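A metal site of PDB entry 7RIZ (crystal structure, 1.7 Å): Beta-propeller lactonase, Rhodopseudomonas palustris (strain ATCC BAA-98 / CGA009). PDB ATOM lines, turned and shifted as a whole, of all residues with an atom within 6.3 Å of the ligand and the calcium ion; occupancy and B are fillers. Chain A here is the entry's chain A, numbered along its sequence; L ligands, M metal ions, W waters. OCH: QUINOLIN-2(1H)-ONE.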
ATOM      1  N   PHE A  13     -15.612  21.537 -24.085  1.00  0.00           N
ATOM      2  CA  PHE A  13     -16.702  22.468 -24.276  1.00  0.00           C
ATOM      3  C   PHE A  13     -16.408  23.726 -23.460  1.00  0.00           C
ATOM      4  O   PHE A  13     -17.064  23.989 -22.442  1.00  0.00           O
ATOM      5  CB  PHE A  13     -18.055  21.900 -23.847  1.00  0.00           C
ATOM      6  CG  PHE A  13     -19.207  22.533 -24.564  1.00  0.00           C
ATOM      7  CD1 PHE A  13     -19.776  23.705 -24.116  1.00  0.00           C
ATOM      8  CD2 PHE A  13     -19.691  21.976 -25.735  1.00  0.00           C
ATOM      9  CE1 PHE A  13     -20.820  24.312 -24.776  1.00  0.00           C
ATOM     10  CE2 PHE A  13     -20.741  22.578 -26.401  1.00  0.00           C
ATOM     11  CZ  PHE A  13     -21.315  23.720 -25.939  1.00  0.00           C
ATOM     12  N   GLU A  15     -16.401  27.600 -22.229  1.00  0.00           N
ATOM     13  CA  GLU A  15     -17.412  28.640 -22.093  1.00  0.00           C
ATOM     14  C   GLU A  15     -16.890  29.593 -21.017  1.00  0.00           C
ATOM     15  O   GLU A  15     -15.813  29.377 -20.458  1.00  0.00           O
ATOM     16  CB  GLU A  15     -18.769  28.069 -21.721  1.00  0.00           C
ATOM     17  CG  GLU A  15     -19.854  28.256 -22.771  1.00  0.00           C
ATOM     18  CD  GLU A  15     -20.655  29.537 -22.582  1.00  0.00           C
ATOM     19  OE1 GLU A  15     -20.173  30.481 -21.924  1.00  0.00           O
ATOM     20  OE2 GLU A  15     -21.797  29.619 -23.112  1.00  0.00           O
ATOM     21  N   ILE A  30     -17.403  22.884 -19.583  1.00  0.00           N
ATOM     22  CA  ILE A  30     -18.658  22.398 -19.041  1.00  0.00           C
ATOM     23  C   ILE A  30     -18.606  20.886 -18.919  1.00  0.00           C
ATOM     24  O   ILE A  30     -19.035  20.315 -17.906  1.00  0.00           O
ATOM     25  CB  ILE A  30     -19.844  22.857 -19.908  1.00  0.00           C
ATOM     26  CG1 ILE A  30     -19.729  24.314 -20.269  1.00  0.00           C
ATOM     27  CG2 ILE A  30     -21.177  22.597 -19.212  1.00  0.00           C
ATOM     28  CD1 ILE A  30     -20.982  24.854 -20.975  1.00  0.00           C
ATOM     29  N   ASN A  55     -20.958  26.873 -16.313  1.00  0.00           N
ATOM     30  CA  ASN A  55     -21.446  27.406 -17.595  1.00  0.00           C
ATOM     31  C   ASN A  55     -20.995  28.839 -17.844  1.00  0.00           C
ATOM     32  O   ASN A  55     -20.792  29.243 -18.990  1.00  0.00           O
ATOM     33  CB  ASN A  55     -22.991  27.358 -17.613  1.00  0.00           C
ATOM     34  CG  ASN A  55     -23.609  27.295 -19.006  1.00  0.00           C
ATOM     35  OD1 ASN A  55     -24.693  26.722 -19.138  1.00  0.00           O
ATOM     36  ND2 ASN A  55     -22.973  27.870 -20.010  1.00  0.00           N
ATOM     37  N   ASN A  70     -25.138  25.125 -14.267  1.00  0.00           N
ATOM     38  CA  ASN A  70     -26.426  24.747 -14.804  1.00  0.00           C
ATOM     39  C   ASN A  70     -26.882  23.386 -14.313  1.00  0.00           C
ATOM     40  O   ASN A  70     -27.947  22.927 -14.719  1.00  0.00           O
ATOM     41  CB  ASN A  70     -26.374  24.790 -16.345  1.00  0.00           C
ATOM     42  CG  ASN A  70     -25.502  23.709 -16.959  1.00  0.00           C
ATOM     43  OD1 ASN A  70     -25.517  22.523 -16.573  1.00  0.00           O
ATOM     44  ND2 ASN A  70     -24.790  24.099 -17.979  1.00  0.00           N
ATOM     45  N   PHE A  73     -25.345  18.544 -17.945  1.00  0.00           N
ATOM     46  CA  PHE A  73     -25.912  18.188 -19.236  1.00  0.00           C
ATOM     47  C   PHE A  73     -25.687  16.699 -19.474  1.00  0.00           C
ATOM     48  O   PHE A  73     -24.778  16.090 -18.902  1.00  0.00           O
ATOM     49  CB  PHE A  73     -25.226  18.975 -20.359  1.00  0.00           C
ATOM     50  CG  PHE A  73     -25.640  20.402 -20.475  1.00  0.00           C
ATOM     51  CD1 PHE A  73     -26.960  20.771 -20.387  1.00  0.00           C
ATOM     52  CD2 PHE A  73     -24.680  21.387 -20.707  1.00  0.00           C
ATOM     53  CE1 PHE A  73     -27.332  22.078 -20.545  1.00  0.00           C
ATOM     54  CE2 PHE A  73     -25.039  22.719 -20.881  1.00  0.00           C
ATOM     55  CZ  PHE A  73     -26.364  23.086 -20.756  1.00  0.00           C
ATOM     56  N   MET A  83     -21.941  17.109 -27.915  1.00  0.00           N
ATOM     57  CA  MET A  83     -22.844  18.245 -27.718  1.00  0.00           C
ATOM     58  C   MET A  83     -23.665  18.078 -26.452  1.00  0.00           C
ATOM     59  O   MET A  83     -24.003  16.962 -26.055  1.00  0.00           O
ATOM     60  CB  MET A  83     -23.784  18.437 -28.913  1.00  0.00           C
ATOM     61  CG  MET A  83     -23.075  18.917 -30.167  1.00  0.00           C
ATOM     62  SD  MET A  83     -22.447  20.606 -30.017  1.00  0.00           S
ATOM     63  CE  MET A  83     -24.004  21.485 -30.107  1.00  0.00           C
ATOM     64  N   PRO A  84     -23.988  19.171 -25.782  1.00  0.00           N
ATOM     65  CA  PRO A  84     -24.857  19.071 -24.612  1.00  0.00           C
ATOM     66  C   PRO A  84     -26.291  18.723 -25.003  1.00  0.00           C
ATOM     67  O   PRO A  84     -26.813  19.161 -26.029  1.00  0.00           O
ATOM     68  CB  PRO A  84     -24.752  20.469 -23.961  1.00  0.00           C
ATOM     69  CG  PRO A  84     -24.343  21.390 -25.073  1.00  0.00           C
ATOM     70  CD  PRO A  84     -23.486  20.539 -25.987  1.00  0.00           C
ATOM     71  N   ASN A 123     -26.839  30.164 -16.479  1.00  0.00           N
ATOM     72  CA  ASN A 123     -26.033  30.156 -17.692  1.00  0.00           C
ATOM     73  C   ASN A 123     -24.897  31.173 -17.692  1.00  0.00           C
ATOM     74  O   ASN A 123     -23.746  30.761 -17.833  1.00  0.00           O
ATOM     75  CB  ASN A 123     -26.941  30.338 -18.936  1.00  0.00           C
ATOM     76  CG  ASN A 123     -26.204  30.068 -20.224  1.00  0.00           C
ATOM     77  OD1 ASN A 123     -25.277  30.757 -20.597  1.00  0.00           O
ATOM     78  ND2 ASN A 123     -26.613  29.032 -20.929  1.00  0.00           N
ATOM     79  N   ASP A 124     -25.187  32.468 -17.672  1.00  0.00           N
ATOM     80  CA  ASP A 124     -24.134  33.479 -17.691  1.00  0.00           C
ATOM     81  C   ASP A 124     -24.497  34.621 -16.745  1.00  0.00           C
ATOM     82  O   ASP A 124     -25.621  34.700 -16.209  1.00  0.00           O
ATOM     83  CB  ASP A 124     -23.904  33.973 -19.114  1.00  0.00           C
ATOM     84  CG  ASP A 124     -22.433  34.310 -19.395  1.00  0.00           C
ATOM     85  OD1 ASP A 124     -21.620  34.381 -18.432  1.00  0.00           O
ATOM     86  OD2 ASP A 124     -22.080  34.454 -20.603  1.00  0.00           O
ATOM     87  N   LEU A 138     -31.135  29.455 -18.300  1.00  0.00           N
ATOM     88  CA  LEU A 138     -31.554  28.867 -19.579  1.00  0.00           C
ATOM     89  C   LEU A 138     -32.674  27.857 -19.423  1.00  0.00           C
ATOM     90  O   LEU A 138     -33.345  27.509 -20.425  1.00  0.00           O
ATOM     91  CB  LEU A 138     -30.370  28.179 -20.236  1.00  0.00           C
ATOM     92  CG  LEU A 138     -30.469  27.746 -21.705  1.00  0.00           C
ATOM     93  CD1 LEU A 138     -30.386  28.923 -22.632  1.00  0.00           C
ATOM     94  CD2 LEU A 138     -29.388  26.723 -22.028  1.00  0.00           C
ATOM     95  N   ARG A 141     -33.722  21.064 -20.259  1.00  0.00           N
ATOM     96  CA  ARG A 141     -34.535  20.246 -21.169  1.00  0.00           C
ATOM     97  C   ARG A 141     -34.840  18.890 -20.528  1.00  0.00           C
ATOM     98  O   ARG A 141     -33.996  18.313 -19.848  1.00  0.00           O
ATOM     99  CB  ARG A 141     -33.787  20.034 -22.486  1.00  0.00           C
ATOM    100  CG  ARG A 141     -33.711  21.261 -23.388  1.00  0.00           C
ATOM    101  CD  ARG A 141     -32.533  21.116 -24.356  1.00  0.00           C
ATOM    102  NE  ARG A 141     -31.258  21.048 -23.622  1.00  0.00           N
ATOM    103  CZ  ARG A 141     -30.079  20.830 -24.196  1.00  0.00           C
ATOM    104  NH1 ARG A 141     -29.978  20.680 -25.515  1.00  0.00           N
ATOM    105  NH2 ARG A 141     -28.994  20.751 -23.431  1.00  0.00           N
ATOM    106  N   ASN A 172     -29.713  33.327 -22.139  1.00  0.00           N
ATOM    107  CA  ASN A 172     -28.354  32.832 -22.262  1.00  0.00           C
ATOM    108  C   ASN A 172     -27.388  33.972 -21.970  1.00  0.00           C
ATOM    109  O   ASN A 172     -27.015  34.207 -20.817  1.00  0.00           O
ATOM    110  CB  ASN A 172     -28.167  32.216 -23.658  1.00  0.00           C
ATOM    111  CG  ASN A 172     -26.957  31.311 -23.736  1.00  0.00           C
ATOM    112  OD1 ASN A 172     -25.888  31.653 -23.278  1.00  0.00           O
ATOM    113  ND2 ASN A 172     -27.109  30.175 -24.433  1.00  0.00           N
ATOM    114  N   GLY A 173     -26.960  34.699 -22.991  1.00  0.00           N
ATOM    115  CA  GLY A 173     -26.059  35.818 -22.751  1.00  0.00           C
ATOM    116  C   GLY A 173     -26.706  36.943 -21.957  1.00  0.00           C
ATOM    117  O   GLY A 173     -27.898  37.219 -22.057  1.00  0.00           O
ATOM    118  N   ASP A 229     -26.068  32.560 -28.148  1.00  0.00           N
ATOM    119  CA  ASP A 229     -25.477  31.982 -26.932  1.00  0.00           C
ATOM    120  C   ASP A 229     -25.132  33.161 -26.028  1.00  0.00           C
ATOM    121  O   ASP A 229     -26.003  33.982 -25.740  1.00  0.00           O
ATOM    122  CB  ASP A 229     -24.291  31.116 -27.292  1.00  0.00           C
ATOM    123  CG  ASP A 229     -23.963  30.111 -26.204  1.00  0.00           C
ATOM    124  OD1 ASP A 229     -24.124  30.386 -24.991  1.00  0.00           O
ATOM    125  OD2 ASP A 229     -23.494  28.994 -26.550  1.00  0.00           O
ATOM    126  N   SER A 230     -23.886  33.289 -25.599  1.00  0.00           N
ATOM    127  CA  SER A 230     -23.527  34.334 -24.651  1.00  0.00           C
ATOM    128  C   SER A 230     -23.016  35.581 -25.360  1.00  0.00           C
ATOM    129  O   SER A 230     -22.899  35.612 -26.582  1.00  0.00           O
ATOM    130  CB  SER A 230     -22.490  33.774 -23.678  1.00  0.00           C
ATOM    131  OG  SER A 230     -23.134  33.053 -22.634  1.00  0.00           O
ATOM    132  N   LEU A 244     -24.999  30.900 -32.846  1.00  0.00           N
ATOM    133  CA  LEU A 244     -24.890  29.494 -33.136  1.00  0.00           C
ATOM    134  C   LEU A 244     -25.481  29.234 -34.506  1.00  0.00           C
ATOM    135  O   LEU A 244     -26.231  30.076 -35.008  1.00  0.00           O
ATOM    136  CB  LEU A 244     -25.655  28.676 -32.093  1.00  0.00           C
ATOM    137  CG  LEU A 244     -25.251  28.957 -30.627  1.00  0.00           C
ATOM    138  CD1 LEU A 244     -26.384  28.555 -29.710  1.00  0.00           C
ATOM    139  CD2 LEU A 244     -23.964  28.211 -30.325  1.00  0.00           C
ATOM    140  N   VAL A 268     -20.783  26.124 -33.398  1.00  0.00           N
ATOM    141  CA  VAL A 268     -21.050  26.202 -31.968  1.00  0.00           C
ATOM    142  C   VAL A 268     -20.139  27.243 -31.336  1.00  0.00           C
ATOM    143  O   VAL A 268     -19.334  26.913 -30.458  1.00  0.00           O
ATOM    144  CB  VAL A 268     -20.849  24.836 -31.279  1.00  0.00           C
ATOM    145  CG1 VAL A 268     -21.486  24.781 -29.952  1.00  0.00           C
ATOM    146  CG2 VAL A 268     -21.429  23.699 -32.192  1.00  0.00           C
ATOM    147  N   THR A 269     -20.261  28.485 -31.779  1.00  0.00           N
ATOM    148  CA  THR A 269     -19.601  29.625 -31.128  1.00  0.00           C
ATOM    149  C   THR A 269     -20.443  30.061 -29.944  1.00  0.00           C
ATOM    150  O   THR A 269     -21.635  30.357 -30.108  1.00  0.00           O
ATOM    151  CB  THR A 269     -19.462  30.752 -32.155  1.00  0.00           C
ATOM    152  OG1 THR A 269     -18.664  30.272 -33.231  1.00  0.00           O
ATOM    153  CG2 THR A 269     -18.802  31.986 -31.523  1.00  0.00           C
ATOM    154  N   THR A 270     -19.814  30.159 -28.718  1.00  0.00           N
ATOM    155  CA  THR A 270     -20.636  30.202 -27.523  1.00  0.00           C
ATOM    156  C   THR A 270     -20.454  31.454 -26.684  1.00  0.00           C
ATOM    157  O   THR A 270     -21.410  31.870 -26.033  1.00  0.00           O
ATOM    158  CB  THR A 270     -20.373  28.979 -26.632  1.00  0.00           C
ATOM    159  OG1 THR A 270     -18.982  28.895 -26.269  1.00  0.00           O
ATOM    160  CG2 THR A 270     -20.789  27.678 -27.353  1.00  0.00           C
ATOM    161  N   ASN A 271     -19.270  32.041 -26.652  1.00  0.00           N
ATOM    162  CA  ASN A 271     -19.088  33.224 -25.815  1.00  0.00           C
ATOM    163  C   ASN A 271     -17.959  34.092 -26.361  1.00  0.00           C
ATOM    164  O   ASN A 271     -17.143  33.666 -27.200  1.00  0.00           O
ATOM    165  CB  ASN A 271     -18.806  32.818 -24.357  1.00  0.00           C
ATOM    166  CG  ASN A 271     -19.334  33.842 -23.323  1.00  0.00           C
ATOM    167  OD1 ASN A 271     -19.363  35.069 -23.533  1.00  0.00           O
ATOM    168  ND2 ASN A 271     -19.790  33.326 -22.209  1.00  0.00           N
ATOM    169  N   SER A 287     -16.844  26.136 -28.981  1.00  0.00           N
ATOM    170  CA  SER A 287     -17.086  24.986 -28.114  1.00  0.00           C
ATOM    171  C   SER A 287     -17.227  23.710 -28.919  1.00  0.00           C
ATOM    172  O   SER A 287     -16.997  22.638 -28.369  1.00  0.00           O
ATOM    173  CB  SER A 287     -18.342  25.218 -27.264  1.00  0.00           C
ATOM    174  OG  SER A 287     -18.128  26.364 -26.392  1.00  0.00           O
HETATM  175  O1  OCH L   1     -24.382  28.321 -22.580  1.00  0.00           O
HETATM  176  N2  OCH L   1     -24.364  27.380 -24.561  1.00  0.00           N
HETATM  177  C3  OCH L   1     -24.737  26.301 -25.355  1.00  0.00           C
HETATM  178  C4  OCH L   1     -24.427  26.284 -26.733  1.00  0.00           C
HETATM  179  C5  OCH L   1     -24.797  25.205 -27.513  1.00  0.00           C
HETATM  180  C6  OCH L   1     -25.494  24.132 -26.955  1.00  0.00           C
HETATM  181  C7  OCH L   1     -25.810  24.149 -25.604  1.00  0.00           C
HETATM  182  C8  OCH L   1     -25.418  25.234 -24.800  1.00  0.00           C
HETATM  183  C9  OCH L   1     -25.734  25.240 -23.471  1.00  0.00           C
HETATM  184  C10 OCH L   1     -25.345  26.308 -22.681  1.00  0.00           C
HETATM  185  C1  OCH L   1     -24.651  27.382 -23.253  1.00  0.00           C
HETATM  186 CA    CA M   1     -23.816  30.736 -22.521  1.00  0.00          CA
HETATM  187  O   HOH W   1     -22.604  31.204 -20.585  1.00  0.00           O
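The calcium ion is bound by water W1 (2.3 Å), OE2 of Glu 15 (2.4 Å), OD1 of Asn 172 (2.4 Å), OD1 of Asn 123 (2.4 Å), OG of Ser 230 (2.4 Å), O1 of the ligand (2.5 Å) and OD1 of Asp 229 (2.5 Å). The calcium ion has seven donor atoms within binding distance.
O1 of the ligand sits close to ND2 of Asn 55, 3.0 Å away.
OE1 of Glu 15 lies within hydrogen-bond range of ND2 of Asn 271 (2.9 Å). The side-chain amide nitrogen (ND2) of Asn 123 lies within hydrogen-bond range of the side-chain amide oxygen (OD1) of Asn 55 (3.5 Å). O of Thr 270 is in hydrogen-bond range of N of Ser 230 (2.9 Å). OD2 of Asp 124 lies close to OG of Ser 230 (2.7 Å). ND2 of Asn 271 lies close to OG of Ser 230 (3.4 Å). The backbone NH (N) of Gly 173 sits at hydrogen-bond distance from the backbone carbonyl oxygen (O) of Asp 229 (3.0 Å). OD1 of Asn 55 is in hydrogen-bond range of ND2 of Asn 70 (2.9 Å). OG1 of Thr 270 sits at hydrogen-bond distance from OG of Ser 287.
Merely in contact with the ligand: Phe 73, Pro 84 and Thr 270. Hydrophobic or aromatic side chains that line the ligand: Phe 73 and Pro 84. Eight residues have an atom within 4 Å of the ligand: Glu 15, Asn 55, Phe 73, Pro 84, Asn 123, Asn 172, Asp 229 and Thr 270. The nearest printed residue that does not touch the ligand is Phe 13 (4.1 Å).
Merely in contact with the calcium ion: Asn 55 (3.9 Å). Along chain A the residues within 4 Å of the calcium ion span positions 15 to 230.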
